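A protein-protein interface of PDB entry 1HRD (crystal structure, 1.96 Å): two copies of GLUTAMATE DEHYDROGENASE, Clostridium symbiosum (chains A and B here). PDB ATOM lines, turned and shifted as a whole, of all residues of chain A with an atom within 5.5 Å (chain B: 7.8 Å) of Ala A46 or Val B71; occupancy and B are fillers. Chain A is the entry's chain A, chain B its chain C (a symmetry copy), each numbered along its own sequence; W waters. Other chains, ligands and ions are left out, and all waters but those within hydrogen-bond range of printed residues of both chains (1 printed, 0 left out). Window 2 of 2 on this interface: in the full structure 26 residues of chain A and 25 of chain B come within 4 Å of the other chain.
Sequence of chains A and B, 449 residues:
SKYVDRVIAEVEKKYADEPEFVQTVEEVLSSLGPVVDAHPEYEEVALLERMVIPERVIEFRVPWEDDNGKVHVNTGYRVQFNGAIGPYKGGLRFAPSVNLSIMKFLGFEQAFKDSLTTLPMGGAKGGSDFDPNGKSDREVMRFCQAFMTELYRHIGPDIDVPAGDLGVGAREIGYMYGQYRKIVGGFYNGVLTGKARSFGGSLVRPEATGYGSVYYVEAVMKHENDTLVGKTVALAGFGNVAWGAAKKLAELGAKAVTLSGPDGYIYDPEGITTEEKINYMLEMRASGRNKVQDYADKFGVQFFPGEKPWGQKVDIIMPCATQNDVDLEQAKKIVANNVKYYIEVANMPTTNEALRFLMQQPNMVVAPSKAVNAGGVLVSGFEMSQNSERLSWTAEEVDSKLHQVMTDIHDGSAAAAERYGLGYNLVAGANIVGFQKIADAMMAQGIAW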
ATOM      1  N   TYR A   3       4.793  -1.374  20.706  1.00  0.00           N
ATOM      2  CA  TYR A   3       5.325  -0.312  19.876  1.00  0.00           C
ATOM      3  C   TYR A   3       6.822  -0.225  20.152  1.00  0.00           C
ATOM      4  O   TYR A   3       7.662  -0.448  19.274  1.00  0.00           O
ATOM      5  CB  TYR A   3       4.555   0.984  20.218  1.00  0.00           C
ATOM      6  CG  TYR A   3       4.946   2.262  19.512  1.00  0.00           C
ATOM      7  CD1 TYR A   3       5.732   2.247  18.358  1.00  0.00           C
ATOM      8  CD2 TYR A   3       4.553   3.503  20.018  1.00  0.00           C
ATOM      9  CE1 TYR A   3       6.108   3.428  17.717  1.00  0.00           C
ATOM     10  CE2 TYR A   3       4.915   4.695  19.392  1.00  0.00           C
ATOM     11  CZ  TYR A   3       5.692   4.656  18.234  1.00  0.00           C
ATOM     12  OH  TYR A   3       6.056   5.821  17.606  1.00  0.00           O
ATOM     13  N   TYR A  42       1.097   8.933  20.376  1.00  0.00           N
ATOM     14  CA  TYR A  42       2.484   9.023  19.964  1.00  0.00           C
ATOM     15  C   TYR A  42       2.730   8.164  18.756  1.00  0.00           C
ATOM     16  O   TYR A  42       3.401   8.499  17.781  1.00  0.00           O
ATOM     17  CB  TYR A  42       3.328   8.359  21.063  1.00  0.00           C
ATOM     18  CG  TYR A  42       3.468   9.239  22.268  1.00  0.00           C
ATOM     19  CD1 TYR A  42       2.962  10.537  22.264  1.00  0.00           C
ATOM     20  CD2 TYR A  42       4.109   8.765  23.412  1.00  0.00           C
ATOM     21  CE1 TYR A  42       3.126  11.373  23.366  1.00  0.00           C
ATOM     22  CE2 TYR A  42       4.267   9.584  24.529  1.00  0.00           C
ATOM     23  CZ  TYR A  42       3.774  10.887  24.503  1.00  0.00           C
ATOM     24  OH  TYR A  42       3.926  11.691  25.604  1.00  0.00           O
ATOM     25  N   GLU A  43       2.187   6.982  18.892  1.00  0.00           N
ATOM     26  CA  GLU A  43       2.377   6.030  17.855  1.00  0.00           C
ATOM     27  C   GLU A  43       1.754   6.360  16.504  1.00  0.00           C
ATOM     28  O   GLU A  43       2.254   5.921  15.470  1.00  0.00           O
ATOM     29  CB  GLU A  43       2.014   4.647  18.373  1.00  0.00           C
ATOM     30  CG  GLU A  43       2.220   3.653  17.250  1.00  0.00           C
ATOM     31  CD  GLU A  43       1.541   2.367  17.566  1.00  0.00           C
ATOM     32  OE1 GLU A  43       0.810   2.421  18.661  1.00  0.00           O
ATOM     33  OE2 GLU A  43       1.694   1.374  16.898  1.00  0.00           O
ATOM     34  N   GLU A  44       0.674   7.137  16.532  1.00  0.00           N
ATOM     35  CA  GLU A  44      -0.094   7.597  15.385  1.00  0.00           C
ATOM     36  C   GLU A  44       0.696   8.573  14.525  1.00  0.00           C
ATOM     37  O   GLU A  44       0.451   8.698  13.323  1.00  0.00           O
ATOM     38  CB  GLU A  44      -1.282   8.409  15.927  1.00  0.00           C
ATOM     39  CG  GLU A  44      -2.630   7.702  16.077  1.00  0.00           C
ATOM     40  CD  GLU A  44      -3.520   8.685  16.793  1.00  0.00           C
ATOM     41  OE1 GLU A  44      -2.906   9.783  17.102  1.00  0.00           O
ATOM     42  OE2 GLU A  44      -4.709   8.462  17.024  1.00  0.00           O
ATOM     43  N   VAL A  45       1.592   9.310  15.179  1.00  0.00           N
ATOM     44  CA  VAL A  45       2.444  10.291  14.529  1.00  0.00           C
ATOM     45  C   VAL A  45       3.868   9.766  14.405  1.00  0.00           C
ATOM     46  O   VAL A  45       4.798  10.549  14.226  1.00  0.00           O
ATOM     47  CB  VAL A  45       2.474  11.646  15.227  1.00  0.00           C
ATOM     48  CG1 VAL A  45       1.100  12.294  15.184  1.00  0.00           C
ATOM     49  CG2 VAL A  45       2.950  11.496  16.668  1.00  0.00           C
ATOM     50  N   ALA A  46       4.051   8.451  14.509  1.00  0.00           N
ATOM     51  CA  ALA A  46       5.367   7.840  14.410  1.00  0.00           C
ATOM     52  C   ALA A  46       6.398   8.559  15.266  1.00  0.00           C
ATOM     53  O   ALA A  46       7.531   8.786  14.854  1.00  0.00           O
ATOM     54  CB  ALA A  46       5.820   7.768  12.957  1.00  0.00           C
ATOM     55  N   LEU A  47       6.005   8.926  16.477  1.00  0.00           N
ATOM     56  CA  LEU A  47       6.908   9.653  17.343  1.00  0.00           C
ATOM     57  C   LEU A  47       8.245   9.003  17.667  1.00  0.00           C
ATOM     58  O   LEU A  47       9.275   9.667  17.615  1.00  0.00           O
ATOM     59  CB  LEU A  47       6.211  10.197  18.594  1.00  0.00           C
ATOM     60  CG  LEU A  47       7.129  11.096  19.405  1.00  0.00           C
ATOM     61  CD1 LEU A  47       6.721  12.552  19.216  1.00  0.00           C
ATOM     62  CD2 LEU A  47       6.988  10.752  20.872  1.00  0.00           C
ATOM     63  N   LEU A  48       8.232   7.725  18.047  1.00  0.00           N
ATOM     64  CA  LEU A  48       9.476   7.060  18.378  1.00  0.00           C
ATOM     65  C   LEU A  48      10.350   6.880  17.147  1.00  0.00           C
ATOM     66  O   LEU A  48      11.574   6.974  17.234  1.00  0.00           O
ATOM     67  CB  LEU A  48       9.304   5.704  19.097  1.00  0.00           C
ATOM     68  CG  LEU A  48       8.526   5.758  20.411  1.00  0.00           C
ATOM     69  CD1 LEU A  48       8.688   4.437  21.154  1.00  0.00           C
ATOM     70  CD2 LEU A  48       8.995   6.911  21.287  1.00  0.00           C
ATOM     71  N   GLU A  49       9.716   6.609  16.008  1.00  0.00           N
ATOM     72  CA  GLU A  49      10.462   6.424  14.778  1.00  0.00           C
ATOM     73  C   GLU A  49      11.248   7.677  14.430  1.00  0.00           C
ATOM     74  O   GLU A  49      12.365   7.616  13.923  1.00  0.00           O
ATOM     75  CB  GLU A  49       9.555   5.945  13.634  1.00  0.00           C
ATOM     76  CG  GLU A  49       8.885   4.586  13.928  1.00  0.00           C
ATOM     77  CD  GLU A  49       7.505   4.680  14.534  1.00  0.00           C
ATOM     78  OE1 GLU A  49       7.416   5.549  15.496  1.00  0.00           O
ATOM     79  OE2 GLU A  49       6.582   3.958  14.173  1.00  0.00           O
ATOM     80  N   ARG A  50      10.647   8.817  14.730  1.00  0.00           N
ATOM     81  CA  ARG A  50      11.293  10.081  14.471  1.00  0.00           C
ATOM     82  C   ARG A  50      12.432  10.351  15.437  1.00  0.00           C
ATOM     83  O   ARG A  50      13.528  10.704  15.014  1.00  0.00           O
ATOM     84  CB  ARG A  50      10.327  11.258  14.481  1.00  0.00           C
ATOM     85  CG  ARG A  50       9.257  11.167  13.393  1.00  0.00           C
ATOM     86  CD  ARG A  50       8.571  12.524  13.296  1.00  0.00           C
ATOM     87  NE  ARG A  50       7.307  12.530  14.008  1.00  0.00           N
ATOM     88  CZ  ARG A  50       6.728  13.539  14.663  1.00  0.00           C
ATOM     89  NH1 ARG A  50       7.249  14.760  14.793  1.00  0.00           N
ATOM     90  NH2 ARG A  50       5.552  13.312  15.237  1.00  0.00           N
ATOM     91  N   MET A  51      12.175  10.179  16.735  1.00  0.00           N
ATOM     92  CA  MET A  51      13.173  10.406  17.768  1.00  0.00           C
ATOM     93  C   MET A  51      14.494   9.675  17.566  1.00  0.00           C
ATOM     94  O   MET A  51      15.529  10.129  18.057  1.00  0.00           O
ATOM     95  CB  MET A  51      12.665  10.065  19.180  1.00  0.00           C
ATOM     96  CG  MET A  51      11.355  10.737  19.545  1.00  0.00           C
ATOM     97  SD  MET A  51      11.126  10.891  21.339  1.00  0.00           S
ATOM     98  CE  MET A  51      12.844  11.097  21.869  1.00  0.00           C
ATOM     99  N   ILE A 447       4.211  17.486  12.573  1.00  0.00           N
ATOM    100  CA  ILE A 447       4.981  16.686  11.642  1.00  0.00           C
ATOM    101  C   ILE A 447       5.746  17.593  10.690  1.00  0.00           C
ATOM    102  O   ILE A 447       5.303  17.817   9.565  1.00  0.00           O
ATOM    103  CB  ILE A 447       4.008  15.841  10.821  1.00  0.00           C
ATOM    104  CG1 ILE A 447       2.967  15.167  11.702  1.00  0.00           C
ATOM    105  CG2 ILE A 447       4.736  14.822   9.964  1.00  0.00           C
ATOM    106  CD1 ILE A 447       3.259  13.698  11.948  1.00  0.00           C
ATOM    107  N   ARG B  61      16.648  13.851   8.821  1.00  0.00           N
ATOM    108  CA  ARG B  61      15.385  13.164   9.007  1.00  0.00           C
ATOM    109  C   ARG B  61      14.335  13.670   8.019  1.00  0.00           C
ATOM    110  O   ARG B  61      14.242  14.875   7.837  1.00  0.00           O
ATOM    111  CB  ARG B  61      14.925  13.501  10.421  1.00  0.00           C
ATOM    112  CG  ARG B  61      13.677  12.758  10.890  1.00  0.00           C
ATOM    113  CD  ARG B  61      13.118  13.339  12.181  1.00  0.00           C
ATOM    114  NE  ARG B  61      14.054  13.232  13.298  1.00  0.00           N
ATOM    115  CZ  ARG B  61      13.917  13.892  14.439  1.00  0.00           C
ATOM    116  NH1 ARG B  61      12.902  14.714  14.656  1.00  0.00           N
ATOM    117  NH2 ARG B  61      14.824  13.723  15.404  1.00  0.00           N
ATOM    118  N   VAL B  62      13.530  12.768   7.444  1.00  0.00           N
ATOM    119  CA  VAL B  62      12.450  13.104   6.518  1.00  0.00           C
ATOM    120  C   VAL B  62      11.153  12.417   6.915  1.00  0.00           C
ATOM    121  O   VAL B  62      10.884  11.281   6.515  1.00  0.00           O
ATOM    122  CB  VAL B  62      12.743  12.826   5.042  1.00  0.00           C
ATOM    123  CG1 VAL B  62      11.694  13.495   4.145  1.00  0.00           C
ATOM    124  CG2 VAL B  62      14.122  13.344   4.674  1.00  0.00           C
ATOM    125  N   PRO B  63      10.355  13.121   7.694  1.00  0.00           N
ATOM    126  CA  PRO B  63       9.069  12.605   8.125  1.00  0.00           C
ATOM    127  C   PRO B  63       8.033  13.055   7.108  1.00  0.00           C
ATOM    128  O   PRO B  63       8.056  14.199   6.657  1.00  0.00           O
ATOM    129  CB  PRO B  63       8.773  13.268   9.475  1.00  0.00           C
ATOM    130  CG  PRO B  63       9.872  14.293   9.742  1.00  0.00           C
ATOM    131  CD  PRO B  63      10.833  14.232   8.556  1.00  0.00           C
ATOM    132  N   TRP B  64       7.117  12.173   6.723  1.00  0.00           N
ATOM    133  CA  TRP B  64       6.125  12.557   5.738  1.00  0.00           C
ATOM    134  C   TRP B  64       4.807  11.820   5.920  1.00  0.00           C
ATOM    135  O   TRP B  64       4.762  10.743   6.512  1.00  0.00           O
ATOM    136  CB  TRP B  64       6.709  12.392   4.326  1.00  0.00           C
ATOM    137  CG  TRP B  64       7.106  10.980   4.039  1.00  0.00           C
ATOM    138  CD1 TRP B  64       8.270  10.371   4.360  1.00  0.00           C
ATOM    139  CD2 TRP B  64       6.308  10.006   3.358  1.00  0.00           C
ATOM    140  NE1 TRP B  64       8.260   9.070   3.916  1.00  0.00           N
ATOM    141  CE2 TRP B  64       7.061   8.821   3.295  1.00  0.00           C
ATOM    142  CE3 TRP B  64       5.038  10.043   2.793  1.00  0.00           C
ATOM    143  CZ2 TRP B  64       6.550   7.675   2.684  1.00  0.00           C
ATOM    144  CZ3 TRP B  64       4.538   8.917   2.192  1.00  0.00           C
ATOM    145  CH2 TRP B  64       5.288   7.743   2.138  1.00  0.00           C
ATOM    146  N   GLU B  65       3.741  12.404   5.397  1.00  0.00           N
ATOM    147  CA  GLU B  65       2.409  11.848   5.556  1.00  0.00           C
ATOM    148  C   GLU B  65       1.860  11.138   4.332  1.00  0.00           C
ATOM    149  O   GLU B  65       1.768  11.732   3.257  1.00  0.00           O
ATOM    150  CB  GLU B  65       1.479  13.021   5.922  1.00  0.00           C
ATOM    151  CG  GLU B  65       0.083  12.567   6.328  1.00  0.00           C
ATOM    152  CD  GLU B  65      -0.880  13.724   6.507  1.00  0.00           C
ATOM    153  OE1 GLU B  65      -0.376  14.893   6.212  1.00  0.00           O
ATOM    154  OE2 GLU B  65      -2.010  13.563   6.926  1.00  0.00           O
ATOM    155  N   ASP B  66       1.424   9.892   4.493  1.00  0.00           N
ATOM    156  CA  ASP B  66       0.844   9.241   3.329  1.00  0.00           C
ATOM    157  C   ASP B  66      -0.609   9.627   3.149  1.00  0.00           C
ATOM    158  O   ASP B  66      -1.172  10.434   3.890  1.00  0.00           O
ATOM    159  CB  ASP B  66       1.040   7.723   3.278  1.00  0.00           C
ATOM    160  CG  ASP B  66       0.135   7.048   4.260  1.00  0.00           C
ATOM    161  OD1 ASP B  66      -0.858   7.609   4.715  1.00  0.00           O
ATOM    162  OD2 ASP B  66       0.547   5.880   4.596  1.00  0.00           O
ATOM    163  N   ASP B  67      -1.212   9.049   2.125  1.00  0.00           N
ATOM    164  CA  ASP B  67      -2.587   9.377   1.814  1.00  0.00           C
ATOM    165  C   ASP B  67      -3.615   8.993   2.856  1.00  0.00           C
ATOM    166  O   ASP B  67      -4.732   9.505   2.846  1.00  0.00           O
ATOM    167  CB  ASP B  67      -3.057   8.901   0.438  1.00  0.00           C
ATOM    168  CG  ASP B  67      -2.313   9.533  -0.701  1.00  0.00           C
ATOM    169  OD1 ASP B  67      -1.816  10.711  -0.453  1.00  0.00           O
ATOM    170  OD2 ASP B  67      -2.263   8.992  -1.800  1.00  0.00           O
ATOM    171  N   ASN B  68      -3.258   8.087   3.744  1.00  0.00           N
ATOM    172  CA  ASN B  68      -4.234   7.733   4.746  1.00  0.00           C
ATOM    173  C   ASN B  68      -3.975   8.513   6.028  1.00  0.00           C
ATOM    174  O   ASN B  68      -4.608   8.274   7.044  1.00  0.00           O
ATOM    175  CB  ASN B  68      -4.347   6.214   4.993  1.00  0.00           C
ATOM    176  CG  ASN B  68      -4.229   5.367   3.739  1.00  0.00           C
ATOM    177  OD1 ASN B  68      -3.336   4.514   3.627  1.00  0.00           O
ATOM    178  ND2 ASN B  68      -5.135   5.589   2.785  1.00  0.00           N
ATOM    179  N   GLY B  69      -3.046   9.459   5.992  1.00  0.00           N
ATOM    180  CA  GLY B  69      -2.760  10.211   7.198  1.00  0.00           C
ATOM    181  C   GLY B  69      -1.761   9.472   8.068  1.00  0.00           C
ATOM    182  O   GLY B  69      -1.466   9.861   9.197  1.00  0.00           O
ATOM    183  N   LYS B  70      -1.239   8.394   7.511  1.00  0.00           N
ATOM    184  CA  LYS B  70      -0.250   7.616   8.213  1.00  0.00           C
ATOM    185  C   LYS B  70       1.124   8.251   8.068  1.00  0.00           C
ATOM    186  O   LYS B  70       1.507   8.652   6.965  1.00  0.00           O
ATOM    187  CB  LYS B  70      -0.242   6.200   7.709  1.00  0.00           C
ATOM    188  CG  LYS B  70       0.849   5.455   8.439  1.00  0.00           C
ATOM    189  CD  LYS B  70       0.319   4.189   9.077  1.00  0.00           C
ATOM    190  CE  LYS B  70       1.085   2.977   8.570  1.00  0.00           C
ATOM    191  NZ  LYS B  70       0.446   2.337   7.408  1.00  0.00           N
ATOM    192  N   VAL B  71       1.860   8.367   9.171  1.00  0.00           N
ATOM    193  CA  VAL B  71       3.172   9.012   9.191  1.00  0.00           C
ATOM    194  C   VAL B  71       4.368   8.082   8.957  1.00  0.00           C
ATOM    195  O   VAL B  71       4.478   7.041   9.603  1.00  0.00           O
ATOM    196  CB  VAL B  71       3.331   9.897  10.420  1.00  0.00           C
ATOM    197  CG1 VAL B  71       4.702  10.567  10.414  1.00  0.00           C
ATOM    198  CG2 VAL B  71       2.248  10.970  10.461  1.00  0.00           C
ATOM    199  N   HIS B  72       5.283   8.452   8.045  1.00  0.00           N
ATOM    200  CA  HIS B  72       6.469   7.646   7.754  1.00  0.00           C
ATOM    201  C   HIS B  72       7.734   8.463   7.969  1.00  0.00           C
ATOM    202  O   HIS B  72       7.666   9.692   7.985  1.00  0.00           O
ATOM    203  CB  HIS B  72       6.493   7.120   6.308  1.00  0.00           C
ATOM    204  CG  HIS B  72       5.254   6.385   5.908  1.00  0.00           C
ATOM    205  ND1 HIS B  72       5.281   5.030   5.622  1.00  0.00           N
ATOM    206  CD2 HIS B  72       3.984   6.837   5.741  1.00  0.00           C
ATOM    207  CE1 HIS B  72       4.042   4.685   5.300  1.00  0.00           C
ATOM    208  NE2 HIS B  72       3.236   5.746   5.364  1.00  0.00           N
ATOM    209  N   VAL B  73       8.887   7.821   8.126  1.00  0.00           N
ATOM    210  CA  VAL B  73      10.116   8.573   8.303  1.00  0.00           C
ATOM    211  C   VAL B  73      11.217   7.949   7.478  1.00  0.00           C
ATOM    212  O   VAL B  73      11.446   6.748   7.566  1.00  0.00           O
ATOM    213  CB  VAL B  73      10.614   8.605   9.738  1.00  0.00           C
ATOM    214  CG1 VAL B  73      11.319   9.928  10.024  1.00  0.00           C
ATOM    215  CG2 VAL B  73       9.464   8.382  10.710  1.00  0.00           C
HETATM  216  O   HOH W   1       1.243   6.482  11.626  1.00  0.00           O
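Among the printed residues, merely in contact across the chains: Val A45 with Val B71 (3.8 Å), Ala A46 with Val B71 (3.7 Å), Glu A49 with Val B73 (3.8 Å), Arg A50 with Pro B63 (3.9 Å), Arg A50 with Val B73 (3.9 Å) and Ile A447 with Val B71 (3.3 Å).
OE1 of Glu A49 is in hydrogen-bond range of OH of Tyr A3 (2.5 Å). The backbone carbonyl oxygen (O) of Val A45 lies within hydrogen-bond range of the guanidinium group (NH2) of Arg A50.
No position is printed for both chains. Of the 7 pairs that touch across the chains among the printed residues, none has its exchanged pair printed and touching as well.
Hydrophobic or aromatic side chains of chain A that line the printed part of chain B: Ala A46 and Ile A447. Printed residues of chain B that touch a printed residue of chain A: Arg B61, Pro B63, Val B71 and Val B73. Hydrophobic or aromatic side chains of chain B that line the printed part of chain A: Pro B63, Val B71 and Val B73. Along chain B the printed residues that touch a printed residue of chain A span positions 61 to 73. Among the printed residues, 7 pairs touch across the chains. Among the printed residues, no Asp or Glu carboxylate lies within 4 Å of a Lys or Arg side-chain nitrogen of the other chain.
Of chain B, only Val B71 comes within 4 Å of Ala A46. Of chain A, only Val A45 (3.8 Å), Ala A46 (3.7 Å) and Ile A447 (3.3 Å) come within 4 Å of Val B71. Printed residues of chain B within 4 Å of Val A45: Val B71. Printed residues of chain B within 4 Å of Ile A447: Val B71 (3.3 Å). Of the printed residues of chain B, Glu A49 touches Val B73. His B72 touches none of the printed residues of chain A. The nearest residue of chain B that does not touch Ala A46 is Val B73 (4.3 Å).
NE of Arg B61 lies within hydrogen-bond range of O of Arg A50 (3.1 Å).
Water W1 bridges the backbone carbonyl oxygen of Glu A44 and the backbone NH of Val B71.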
